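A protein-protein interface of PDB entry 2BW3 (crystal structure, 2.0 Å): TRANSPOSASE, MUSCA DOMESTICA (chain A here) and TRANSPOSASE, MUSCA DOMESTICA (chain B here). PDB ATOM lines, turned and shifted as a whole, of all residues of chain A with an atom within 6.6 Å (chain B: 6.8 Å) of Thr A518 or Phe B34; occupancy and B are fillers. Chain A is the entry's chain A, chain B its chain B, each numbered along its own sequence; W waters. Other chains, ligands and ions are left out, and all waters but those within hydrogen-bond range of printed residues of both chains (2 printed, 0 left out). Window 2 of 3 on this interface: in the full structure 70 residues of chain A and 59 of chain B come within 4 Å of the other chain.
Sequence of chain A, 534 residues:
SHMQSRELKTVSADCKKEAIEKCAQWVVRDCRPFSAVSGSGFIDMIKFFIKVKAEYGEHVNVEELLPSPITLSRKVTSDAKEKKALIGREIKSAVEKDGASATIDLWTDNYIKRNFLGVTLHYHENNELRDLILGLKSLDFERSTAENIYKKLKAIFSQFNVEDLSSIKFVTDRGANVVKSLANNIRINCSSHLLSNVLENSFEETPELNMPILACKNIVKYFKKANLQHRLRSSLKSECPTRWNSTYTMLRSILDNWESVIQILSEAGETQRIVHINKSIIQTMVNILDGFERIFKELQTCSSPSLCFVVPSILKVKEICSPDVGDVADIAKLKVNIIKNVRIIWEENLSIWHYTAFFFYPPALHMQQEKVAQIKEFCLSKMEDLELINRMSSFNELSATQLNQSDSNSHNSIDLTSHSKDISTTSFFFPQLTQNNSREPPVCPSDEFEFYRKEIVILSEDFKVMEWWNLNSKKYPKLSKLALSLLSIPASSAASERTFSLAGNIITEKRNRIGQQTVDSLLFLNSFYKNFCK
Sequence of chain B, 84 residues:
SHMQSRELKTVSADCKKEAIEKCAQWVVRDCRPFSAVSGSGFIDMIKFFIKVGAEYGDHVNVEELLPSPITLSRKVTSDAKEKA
OG1 of Thr A77 is in hydrogen-bond range of O of Ser A73, at 3.3 Å. O of Ile A506 sits at hydrogen-bond distance from N of Ile A514 (2.9 Å). O of Gly A515 lies within hydrogen-bond range of OG1 of Thr A518 (2.9 Å). The backbone carbonyl oxygen (O) of Val B27 lies within hydrogen-bond range of the backbone NH (N) of Arg B32 (3.1 Å). The side-chain hydroxyl (OG) of Ser B38 lies within hydrogen-bond range of the backbone carbonyl oxygen (O) of Ser B35, at 2.9 Å.
Water W2 bridges the side-chain hydroxyl (OG) of Ser B35 (2.6 Å) and the side-chain amide oxygen (OD1) of Asn A512 (2.7 Å). Water W1 lies within hydrogen-bond range of O of Val B37 (2.8 Å) and O of Pro A67 (2.8 Å).
Among the printed residues, pairs that only touch across the chains: Pro A67 with Val B37 (3.5 Å), Pro A69 with Phe B34 (3.6 Å), Pro A69 with Val B37 (3.8 Å), Pro A69 with Ser B38 (3.99 Å), Leu A72 with Ala B24 (3.7 Å), Leu A72 with Phe B34 (3.9 Å), Leu A72 with Val B37 (3.4 Å), Ser A73 with Phe B34 (3.7 Å), Val A76 with Val B28 (3.6 Å), Val A76 with Phe B34 (3.7 Å), Ile A506 with Arg B32 (3.7 Å), Ile A506 with Pro B33 (3.5 Å), Asn A512 with Pro B33 (3.2 Å), Ile A514 with Phe B34 (3.6 Å), Thr A518 with Phe B34 (3.97 Å), Leu A522 with Val B27 (3.9 Å) and Leu A522 with Val B28 (3.7 Å).
Of the printed residues of chain B, Pro A67 touches Val B37. Printed residues of chain B within 4 Å of Leu A72: Ala B24, Phe B34 and Val B37. Printed residues of chain B within 4 Å of Ser A73: Phe B34. Thr A518 touches just one residue of chain B: Phe B34 (3.97 Å). Printed residues of chain A within 4 Å of Ala B24: Leu A72. Phe B34 touches six residues of chain A. Printed residues of chain A within 4 Å of Val B37: Pro A67, Pro A69 and Leu A72. The nearest printed residue of chain B that does not touch Thr A518 is Val B28 (7.3 Å). The nearest residue of chain A that does not touch Phe B34 is Leu A522 (4.7 Å).
Of the 11 printed residues of chain B, 8 touch a printed residue of chain A. Hydrophobic or aromatic side chains of chain B within 4 Å of the printed part of chain A: Val B28, Pro B33, Phe B34 and Val B37. Of the 22 printed residues of chain A, 10 touch a printed residue of chain B. Hydrophobic or aromatic side chains of chain A that line the printed part of chain B: Pro A69, Leu A72, Val A76, Ile A506, Ile A514 and Leu A522. Along chain A the printed residues that touch a printed residue of chain B span positions 67 to 522. Among the printed residues, 17 pairs touch across the chains.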
ATOM      1  N   PRO A  67       6.337   2.106  19.598  1.00  0.00           N
ATOM      2  CA  PRO A  67       5.377   1.491  18.680  1.00  0.00           C
ATOM      3  C   PRO A  67       4.562   2.634  18.048  1.00  0.00           C
ATOM      4  O   PRO A  67       4.486   3.743  18.595  1.00  0.00           O
ATOM      5  CB  PRO A  67       4.503   0.651  19.614  1.00  0.00           C
ATOM      6  CG  PRO A  67       4.566   1.409  20.918  1.00  0.00           C
ATOM      7  CD  PRO A  67       6.018   1.800  21.011  1.00  0.00           C
ATOM      8  N   SER A  68       3.960   2.368  16.904  1.00  0.00           N
ATOM      9  CA  SER A  68       3.113   3.348  16.234  1.00  0.00           C
ATOM     10  C   SER A  68       1.719   3.217  16.864  1.00  0.00           C
ATOM     11  O   SER A  68       1.411   2.187  17.452  1.00  0.00           O
ATOM     12  CB  SER A  68       2.984   2.950  14.765  1.00  0.00           C
ATOM     13  OG  SER A  68       2.277   1.720  14.676  1.00  0.00           O
ATOM     14  N   PRO A  69       0.851   4.221  16.680  1.00  0.00           N
ATOM     15  CA  PRO A  69      -0.527   4.235  17.206  1.00  0.00           C
ATOM     16  C   PRO A  69      -1.283   2.999  16.691  1.00  0.00           C
ATOM     17  O   PRO A  69      -2.099   2.404  17.402  1.00  0.00           O
ATOM     18  CB  PRO A  69      -1.116   5.492  16.570  1.00  0.00           C
ATOM     19  CG  PRO A  69       0.067   6.434  16.565  1.00  0.00           C
ATOM     20  CD  PRO A  69       1.227   5.541  16.117  1.00  0.00           C
ATOM     21  N   ILE A  70      -1.002   2.635  15.443  1.00  0.00           N
ATOM     22  CA  ILE A  70      -1.623   1.478  14.762  1.00  0.00           C
ATOM     23  C   ILE A  70      -1.272   0.166  15.469  1.00  0.00           C
ATOM     24  O   ILE A  70      -2.136  -0.682  15.706  1.00  0.00           O
ATOM     25  CB  ILE A  70      -1.127   1.373  13.259  1.00  0.00           C
ATOM     26  CG1 ILE A  70      -1.608   2.581  12.452  1.00  0.00           C
ATOM     27  CG2 ILE A  70      -1.629   0.052  12.582  1.00  0.00           C
ATOM     28  CD1 ILE A  70      -3.083   2.812  12.567  1.00  0.00           C
ATOM     29  N   LEU A  72      -0.323  -0.161  18.525  1.00  0.00           N
ATOM     30  CA  LEU A  72      -0.942  -0.112  19.865  1.00  0.00           C
ATOM     31  C   LEU A  72      -2.393  -0.469  19.783  1.00  0.00           C
ATOM     32  O   LEU A  72      -2.897  -1.207  20.619  1.00  0.00           O
ATOM     33  CB  LEU A  72      -0.788   1.274  20.505  1.00  0.00           C
ATOM     34  CG  LEU A  72       0.640   1.698  20.874  1.00  0.00           C
ATOM     35  CD1 LEU A  72       0.557   3.041  21.683  1.00  0.00           C
ATOM     36  CD2 LEU A  72       1.330   0.608  21.729  1.00  0.00           C
ATOM     37  N   SER A  73      -3.076   0.045  18.762  1.00  0.00           N
ATOM     38  CA  SER A  73      -4.472  -0.281  18.586  1.00  0.00           C
ATOM     39  C   SER A  73      -4.632  -1.797  18.432  1.00  0.00           C
ATOM     40  O   SER A  73      -5.460  -2.426  19.120  1.00  0.00           O
ATOM     41  CB  SER A  73      -5.027   0.427  17.362  1.00  0.00           C
ATOM     42  OG  SER A  73      -6.404   0.218  17.285  1.00  0.00           O
ATOM     43  N   ARG A  74      -3.849  -2.403  17.543  1.00  0.00           N
ATOM     44  CA  ARG A  74      -3.921  -3.872  17.379  1.00  0.00           C
ATOM     45  C   ARG A  74      -3.648  -4.611  18.677  1.00  0.00           C
ATOM     46  O   ARG A  74      -4.260  -5.660  18.944  1.00  0.00           O
ATOM     47  CB  ARG A  74      -2.874  -4.421  16.397  1.00  0.00           C
ATOM     48  CG  ARG A  74      -3.224  -4.386  14.952  1.00  0.00           C
ATOM     49  CD  ARG A  74      -2.476  -5.505  14.202  1.00  0.00           C
ATOM     50  NE  ARG A  74      -1.013  -5.427  14.334  1.00  0.00           N
ATOM     51  CZ  ARG A  74      -0.270  -4.519  13.715  1.00  0.00           C
ATOM     52  NH1 ARG A  74      -0.859  -3.595  12.949  1.00  0.00           N
ATOM     53  NH2 ARG A  74       1.060  -4.633  13.728  1.00  0.00           N
ATOM     54  N   VAL A  76      -4.072  -3.610  21.867  1.00  0.00           N
ATOM     55  CA  VAL A  76      -5.180  -3.488  22.808  1.00  0.00           C
ATOM     56  C   VAL A  76      -6.282  -4.484  22.392  1.00  0.00           C
ATOM     57  O   VAL A  76      -6.797  -5.235  23.232  1.00  0.00           O
ATOM     58  CB  VAL A  76      -5.702  -2.035  22.858  1.00  0.00           C
ATOM     59  CG1 VAL A  76      -7.037  -1.958  23.606  1.00  0.00           C
ATOM     60  CG2 VAL A  76      -4.662  -1.150  23.566  1.00  0.00           C
ATOM     61  N   THR A  77      -6.603  -4.504  21.099  1.00  0.00           N
ATOM     62  CA  THR A  77      -7.606  -5.410  20.576  1.00  0.00           C
ATOM     63  C   THR A  77      -7.241  -6.872  20.831  1.00  0.00           C
ATOM     64  O   THR A  77      -8.051  -7.627  21.374  1.00  0.00           O
ATOM     65  CB  THR A  77      -7.843  -5.128  19.094  1.00  0.00           C
ATOM     66  OG1 THR A  77      -8.472  -3.844  18.974  1.00  0.00           O
ATOM     67  CG2 THR A  77      -8.747  -6.229  18.449  1.00  0.00           C
ATOM     68  N   ILE A 506     -11.183   9.932  24.907  1.00  0.00           N
ATOM     69  CA  ILE A 506     -11.085   8.997  23.808  1.00  0.00           C
ATOM     70  C   ILE A 506     -12.416   8.623  23.136  1.00  0.00           C
ATOM     71  O   ILE A 506     -12.433   7.925  22.112  1.00  0.00           O
ATOM     72  CB  ILE A 506     -10.299   7.759  24.217  1.00  0.00           C
ATOM     73  CG1 ILE A 506     -10.949   7.085  25.427  1.00  0.00           C
ATOM     74  CG2 ILE A 506      -8.848   8.158  24.473  1.00  0.00           C
ATOM     75  CD1 ILE A 506     -10.388   5.721  25.744  1.00  0.00           C
ATOM     76  N   ASN A 512      -8.505  12.897  19.410  1.00  0.00           N
ATOM     77  CA  ASN A 512      -8.175  11.803  20.340  1.00  0.00           C
ATOM     78  C   ASN A 512      -9.108  10.612  20.367  1.00  0.00           C
ATOM     79  O   ASN A 512      -8.799   9.600  20.993  1.00  0.00           O
ATOM     80  CB  ASN A 512      -8.084  12.364  21.760  1.00  0.00           C
ATOM     81  CG  ASN A 512      -7.065  13.464  21.863  1.00  0.00           C
ATOM     82  OD1 ASN A 512      -5.985  13.399  21.247  1.00  0.00           O
ATOM     83  ND2 ASN A 512      -7.398  14.496  22.610  1.00  0.00           N
ATOM     84  N   ARG A 513     -10.194  10.722  19.619  1.00  0.00           N
ATOM     85  CA  ARG A 513     -11.246   9.733  19.548  1.00  0.00           C
ATOM     86  C   ARG A 513     -10.840   8.367  18.945  1.00  0.00           C
ATOM     87  O   ARG A 513     -10.322   8.298  17.834  1.00  0.00           O
ATOM     88  CB  ARG A 513     -12.399  10.358  18.733  1.00  0.00           C
ATOM     89  CG  ARG A 513     -13.669   9.535  18.647  1.00  0.00           C
ATOM     90  CD  ARG A 513     -14.671  10.188  17.690  1.00  0.00           C
ATOM     91  NE  ARG A 513     -15.525   9.158  17.096  1.00  0.00           N
ATOM     92  CZ  ARG A 513     -15.852   9.084  15.808  1.00  0.00           C
ATOM     93  NH1 ARG A 513     -15.416   9.990  14.947  1.00  0.00           N
ATOM     94  NH2 ARG A 513     -16.598   8.073  15.374  1.00  0.00           N
ATOM     95  N   ILE A 514     -11.074   7.287  19.673  1.00  0.00           N
ATOM     96  CA  ILE A 514     -10.756   5.981  19.099  1.00  0.00           C
ATOM     97  C   ILE A 514     -12.072   5.323  18.641  1.00  0.00           C
ATOM     98  O   ILE A 514     -13.157   5.753  19.027  1.00  0.00           O
ATOM     99  CB  ILE A 514      -9.913   5.093  20.063  1.00  0.00           C
ATOM    100  CG1 ILE A 514     -10.722   4.662  21.280  1.00  0.00           C
ATOM    101  CG2 ILE A 514      -8.637   5.847  20.505  1.00  0.00           C
ATOM    102  CD1 ILE A 514      -9.914   3.839  22.259  1.00  0.00           C
ATOM    103  N   GLY A 515     -11.987   4.312  17.799  1.00  0.00           N
ATOM    104  CA  GLY A 515     -13.208   3.693  17.306  1.00  0.00           C
ATOM    105  C   GLY A 515     -14.003   2.929  18.343  1.00  0.00           C
ATOM    106  O   GLY A 515     -13.437   2.466  19.335  1.00  0.00           O
ATOM    107  N   GLN A 516     -15.291   2.738  18.062  1.00  0.00           N
ATOM    108  CA  GLN A 516     -16.212   2.021  18.959  1.00  0.00           C
ATOM    109  C   GLN A 516     -15.703   0.662  19.468  1.00  0.00           C
ATOM    110  O   GLN A 516     -15.741   0.408  20.661  1.00  0.00           O
ATOM    111  CB  GLN A 516     -17.581   1.832  18.281  1.00  0.00           C
ATOM    112  CG  GLN A 516     -18.591   1.043  19.126  1.00  0.00           C
ATOM    113  CD  GLN A 516     -18.922   1.790  20.393  1.00  0.00           C
ATOM    114  OE1 GLN A 516     -19.501   2.867  20.343  1.00  0.00           O
ATOM    115  NE2 GLN A 516     -18.502   1.248  21.538  1.00  0.00           N
ATOM    116  N   GLN A 517     -15.238  -0.210  18.574  1.00  0.00           N
ATOM    117  CA  GLN A 517     -14.744  -1.523  18.993  1.00  0.00           C
ATOM    118  C   GLN A 517     -13.574  -1.404  19.973  1.00  0.00           C
ATOM    119  O   GLN A 517     -13.528  -2.149  20.969  1.00  0.00           O
ATOM    120  CB  GLN A 517     -14.313  -2.396  17.798  1.00  0.00           C
ATOM    121  CG  GLN A 517     -15.345  -2.544  16.679  1.00  0.00           C
ATOM    122  CD  GLN A 517     -16.738  -2.767  17.229  1.00  0.00           C
ATOM    123  OE1 GLN A 517     -16.999  -3.787  17.863  1.00  0.00           O
ATOM    124  NE2 GLN A 517     -17.630  -1.796  17.019  1.00  0.00           N
ATOM    125  N   THR A 518     -12.612  -0.511  19.692  1.00  0.00           N
ATOM    126  CA  THR A 518     -11.454  -0.368  20.588  1.00  0.00           C
ATOM    127  C   THR A 518     -11.815   0.300  21.894  1.00  0.00           C
ATOM    128  O   THR A 518     -11.149   0.051  22.891  1.00  0.00           O
ATOM    129  CB  THR A 518     -10.260   0.359  19.948  1.00  0.00           C
ATOM    130  OG1 THR A 518     -10.712   1.597  19.420  1.00  0.00           O
ATOM    131  CG2 THR A 518      -9.706  -0.470  18.826  1.00  0.00           C
ATOM    132  N   VAL A 519     -12.838   1.156  21.885  1.00  0.00           N
ATOM    133  CA  VAL A 519     -13.321   1.763  23.133  1.00  0.00           C
ATOM    134  C   VAL A 519     -13.794   0.608  24.039  1.00  0.00           C
ATOM    135  O   VAL A 519     -13.473   0.556  25.218  1.00  0.00           O
ATOM    136  CB  VAL A 519     -14.547   2.695  22.877  1.00  0.00           C
ATOM    137  CG1 VAL A 519     -15.273   3.034  24.197  1.00  0.00           C
ATOM    138  CG2 VAL A 519     -14.107   3.979  22.196  1.00  0.00           C
ATOM    139  N   ASP A 520     -14.550  -0.329  23.474  1.00  0.00           N
ATOM    140  CA  ASP A 520     -15.055  -1.463  24.262  1.00  0.00           C
ATOM    141  C   ASP A 520     -13.918  -2.343  24.736  1.00  0.00           C
ATOM    142  O   ASP A 520     -13.892  -2.757  25.894  1.00  0.00           O
ATOM    143  CB  ASP A 520     -16.056  -2.323  23.447  1.00  0.00           C
ATOM    144  CG  ASP A 520     -17.338  -1.563  23.065  1.00  0.00           C
ATOM    145  OD1 ASP A 520     -17.767  -0.646  23.799  1.00  0.00           O
ATOM    146  OD2 ASP A 520     -17.926  -1.886  22.014  1.00  0.00           O
ATOM    147  N   SER A 521     -12.949  -2.598  23.857  1.00  0.00           N
ATOM    148  CA  SER A 521     -11.803  -3.404  24.215  1.00  0.00           C
ATOM    149  C   SER A 521     -10.967  -2.704  25.296  1.00  0.00           C
ATOM    150  O   SER A 521     -10.506  -3.328  26.258  1.00  0.00           O
ATOM    151  CB  SER A 521     -10.916  -3.638  22.986  1.00  0.00           C
ATOM    152  OG  SER A 521     -11.528  -4.526  22.076  1.00  0.00           O
ATOM    153  N   LEU A 522     -10.804  -1.399  25.156  1.00  0.00           N
ATOM    154  CA  LEU A 522      -9.987  -0.682  26.116  1.00  0.00           C
ATOM    155  C   LEU A 522     -10.611  -0.635  27.513  1.00  0.00           C
ATOM    156  O   LEU A 522      -9.935  -0.905  28.509  1.00  0.00           O
ATOM    157  CB  LEU A 522      -9.688   0.717  25.606  1.00  0.00           C
ATOM    158  CG  LEU A 522      -8.658   1.550  26.359  1.00  0.00           C
ATOM    159  CD1 LEU A 522      -7.999   2.531  25.391  1.00  0.00           C
ATOM    160  CD2 LEU A 522      -9.309   2.288  27.488  1.00  0.00           C
ATOM    161  N   LEU A 523     -11.909  -0.380  27.565  1.00  0.00           N
ATOM    162  CA  LEU A 523     -12.651  -0.305  28.841  1.00  0.00           C
ATOM    163  C   LEU A 523     -12.695  -1.664  29.543  1.00  0.00           C
ATOM    164  O   LEU A 523     -12.528  -1.762  30.782  1.00  0.00           O
ATOM    165  CB  LEU A 523     -14.070   0.240  28.579  1.00  0.00           C
ATOM    166  CG  LEU A 523     -14.226   1.763  28.727  1.00  0.00           C
ATOM    167  CD1 LEU A 523     -13.020   2.490  28.311  1.00  0.00           C
ATOM    168  CD2 LEU A 523     -15.438   2.273  27.997  1.00  0.00           C
ATOM    169  N   ALA B  24       0.931   0.127  25.401  1.00  0.00           N
ATOM    170  CA  ALA B  24      -0.468  -0.309  25.323  1.00  0.00           C
ATOM    171  C   ALA B  24      -1.106  -0.232  26.729  1.00  0.00           C
ATOM    172  O   ALA B  24      -2.203   0.275  26.874  1.00  0.00           O
ATOM    173  CB  ALA B  24      -0.567  -1.763  24.772  1.00  0.00           C
ATOM    174  N   TRP B  26      -0.192   1.676  29.118  1.00  0.00           N
ATOM    175  CA  TRP B  26      -0.323   3.097  29.446  1.00  0.00           C
ATOM    176  C   TRP B  26      -1.656   3.638  28.916  1.00  0.00           C
ATOM    177  O   TRP B  26      -2.425   4.222  29.666  1.00  0.00           O
ATOM    178  CB  TRP B  26       0.824   3.874  28.819  1.00  0.00           C
ATOM    179  CG  TRP B  26       0.629   5.366  28.833  1.00  0.00           C
ATOM    180  CD1 TRP B  26       0.146   6.134  29.861  1.00  0.00           C
ATOM    181  CD2 TRP B  26       0.938   6.264  27.775  1.00  0.00           C
ATOM    182  NE1 TRP B  26       0.142   7.448  29.501  1.00  0.00           N
ATOM    183  CE2 TRP B  26       0.616   7.560  28.223  1.00  0.00           C
ATOM    184  CE3 TRP B  26       1.457   6.098  26.485  1.00  0.00           C
ATOM    185  CZ2 TRP B  26       0.797   8.701  27.427  1.00  0.00           C
ATOM    186  CZ3 TRP B  26       1.642   7.247  25.686  1.00  0.00           C
ATOM    187  CH2 TRP B  26       1.309   8.522  26.168  1.00  0.00           C
ATOM    188  N   VAL B  27      -1.939   3.455  27.626  1.00  0.00           N
ATOM    189  CA  VAL B  27      -3.186   3.973  27.077  1.00  0.00           C
ATOM    190  C   VAL B  27      -4.446   3.306  27.658  1.00  0.00           C
ATOM    191  O   VAL B  27      -5.434   3.985  27.895  1.00  0.00           O
ATOM    192  CB  VAL B  27      -3.218   3.938  25.540  1.00  0.00           C
ATOM    193  CG1 VAL B  27      -1.995   4.691  24.949  1.00  0.00           C
ATOM    194  CG2 VAL B  27      -3.298   2.534  25.040  1.00  0.00           C
ATOM    195  N   VAL B  28      -4.378   2.028  27.977  1.00  0.00           N
ATOM    196  CA  VAL B  28      -5.527   1.316  28.571  1.00  0.00           C
ATOM    197  C   VAL B  28      -5.781   1.789  30.030  1.00  0.00           C
ATOM    198  O   VAL B  28      -6.906   2.165  30.402  1.00  0.00           O
ATOM    199  CB  VAL B  28      -5.252  -0.211  28.574  1.00  0.00           C
ATOM    200  CG1 VAL B  28      -6.314  -0.939  29.415  1.00  0.00           C
ATOM    201  CG2 VAL B  28      -5.259  -0.744  27.129  1.00  0.00           C
ATOM    202  N   ARG B  32      -5.720   7.045  27.387  1.00  0.00           N
ATOM    203  CA  ARG B  32      -5.056   7.973  26.468  1.00  0.00           C
ATOM    204  C   ARG B  32      -5.303   7.488  25.045  1.00  0.00           C
ATOM    205  O   ARG B  32      -5.446   6.288  24.824  1.00  0.00           O
ATOM    206  CB  ARG B  32      -3.548   7.950  26.706  1.00  0.00           C
ATOM    207  CG  ARG B  32      -3.124   8.410  28.113  1.00  0.00           C
ATOM    208  CD  ARG B  32      -3.478   9.886  28.358  1.00  0.00           C
ATOM    209  NE  ARG B  32      -3.498  10.163  29.796  1.00  0.00           N
ATOM    210  CZ  ARG B  32      -4.362  10.969  30.390  1.00  0.00           C
ATOM    211  NH1 ARG B  32      -5.289  11.589  29.667  1.00  0.00           N
ATOM    212  NH2 ARG B  32      -4.324  11.122  31.710  1.00  0.00           N
ATOM    213  N   PRO B  33      -5.363   8.415  24.064  1.00  0.00           N
ATOM    214  CA  PRO B  33      -5.579   8.039  22.673  1.00  0.00           C
ATOM    215  C   PRO B  33      -4.331   7.312  22.159  1.00  0.00           C
ATOM    216  O   PRO B  33      -3.231   7.588  22.622  1.00  0.00           O
ATOM    217  CB  PRO B  33      -5.717   9.396  21.980  1.00  0.00           C
ATOM    218  CG  PRO B  33      -4.858  10.312  22.844  1.00  0.00           C
ATOM    219  CD  PRO B  33      -5.255   9.883  24.214  1.00  0.00           C
ATOM    220  N   PHE B  34      -4.489   6.438  21.170  1.00  0.00           N
ATOM    221  CA  PHE B  34      -3.321   5.733  20.597  1.00  0.00           C
ATOM    222  C   PHE B  34      -2.348   6.756  19.984  1.00  0.00           C
ATOM    223  O   PHE B  34      -1.104   6.558  19.957  1.00  0.00           O
ATOM    224  CB  PHE B  34      -3.791   4.774  19.510  1.00  0.00           C
ATOM    225  CG  PHE B  34      -4.740   3.710  20.009  1.00  0.00           C
ATOM    226  CD1 PHE B  34      -6.027   3.615  19.502  1.00  0.00           C
ATOM    227  CD2 PHE B  34      -4.346   2.824  21.001  1.00  0.00           C
ATOM    228  CE1 PHE B  34      -6.927   2.643  19.982  1.00  0.00           C
ATOM    229  CE2 PHE B  34      -5.246   1.848  21.486  1.00  0.00           C
ATOM    230  CZ  PHE B  34      -6.534   1.767  20.970  1.00  0.00           C
ATOM    231  N   SER B  35      -2.907   7.852  19.477  1.00  0.00           N
ATOM    232  CA  SER B  35      -2.079   8.915  18.888  1.00  0.00           C
ATOM    233  C   SER B  35      -1.139   9.637  19.856  1.00  0.00           C
ATOM    234  O   SER B  35      -0.278  10.407  19.412  1.00  0.00           O
ATOM    235  CB  SER B  35      -2.966   9.952  18.190  1.00  0.00           C
ATOM    236  OG  SER B  35      -3.981  10.418  19.057  1.00  0.00           O
ATOM    237  N   ALA B  36      -1.277   9.404  21.164  1.00  0.00           N
ATOM    238  CA  ALA B  36      -0.391  10.073  22.123  1.00  0.00           C
ATOM    239  C   ALA B  36       1.079   9.650  21.939  1.00  0.00           C
ATOM    240  O   ALA B  36       2.015  10.430  22.256  1.00  0.00           O
ATOM    241  CB  ALA B  36      -0.842   9.799  23.553  1.00  0.00           C
ATOM    242  N   VAL B  37       1.303   8.455  21.386  1.00  0.00           N
ATOM    243  CA  VAL B  37       2.694   8.002  21.212  1.00  0.00           C
ATOM    244  C   VAL B  37       3.433   8.596  20.037  1.00  0.00           C
ATOM    245  O   VAL B  37       4.618   8.307  19.861  1.00  0.00           O
ATOM    246  CB  VAL B  37       2.873   6.464  21.053  1.00  0.00           C
ATOM    247  CG1 VAL B  37       2.572   5.769  22.314  1.00  0.00           C
ATOM    248  CG2 VAL B  37       2.106   5.940  19.855  1.00  0.00           C
ATOM    249  N   SER B  38       2.739   9.326  19.180  1.00  0.00           N
ATOM    250  CA  SER B  38       3.409   9.909  18.024  1.00  0.00           C
ATOM    251  C   SER B  38       3.698  11.403  18.228  1.00  0.00           C
ATOM    252  O   SER B  38       4.314  12.061  17.388  1.00  0.00           O
ATOM    253  CB  SER B  38       2.554   9.681  16.776  1.00  0.00           C
ATOM    254  OG  SER B  38       1.273  10.219  16.968  1.00  0.00           O
HETATM  255  O   HOH W   1       5.232   6.376  17.905  1.00  0.00           O
HETATM  256  O   HOH W   2      -3.784  12.860  19.807  1.00  0.00           O
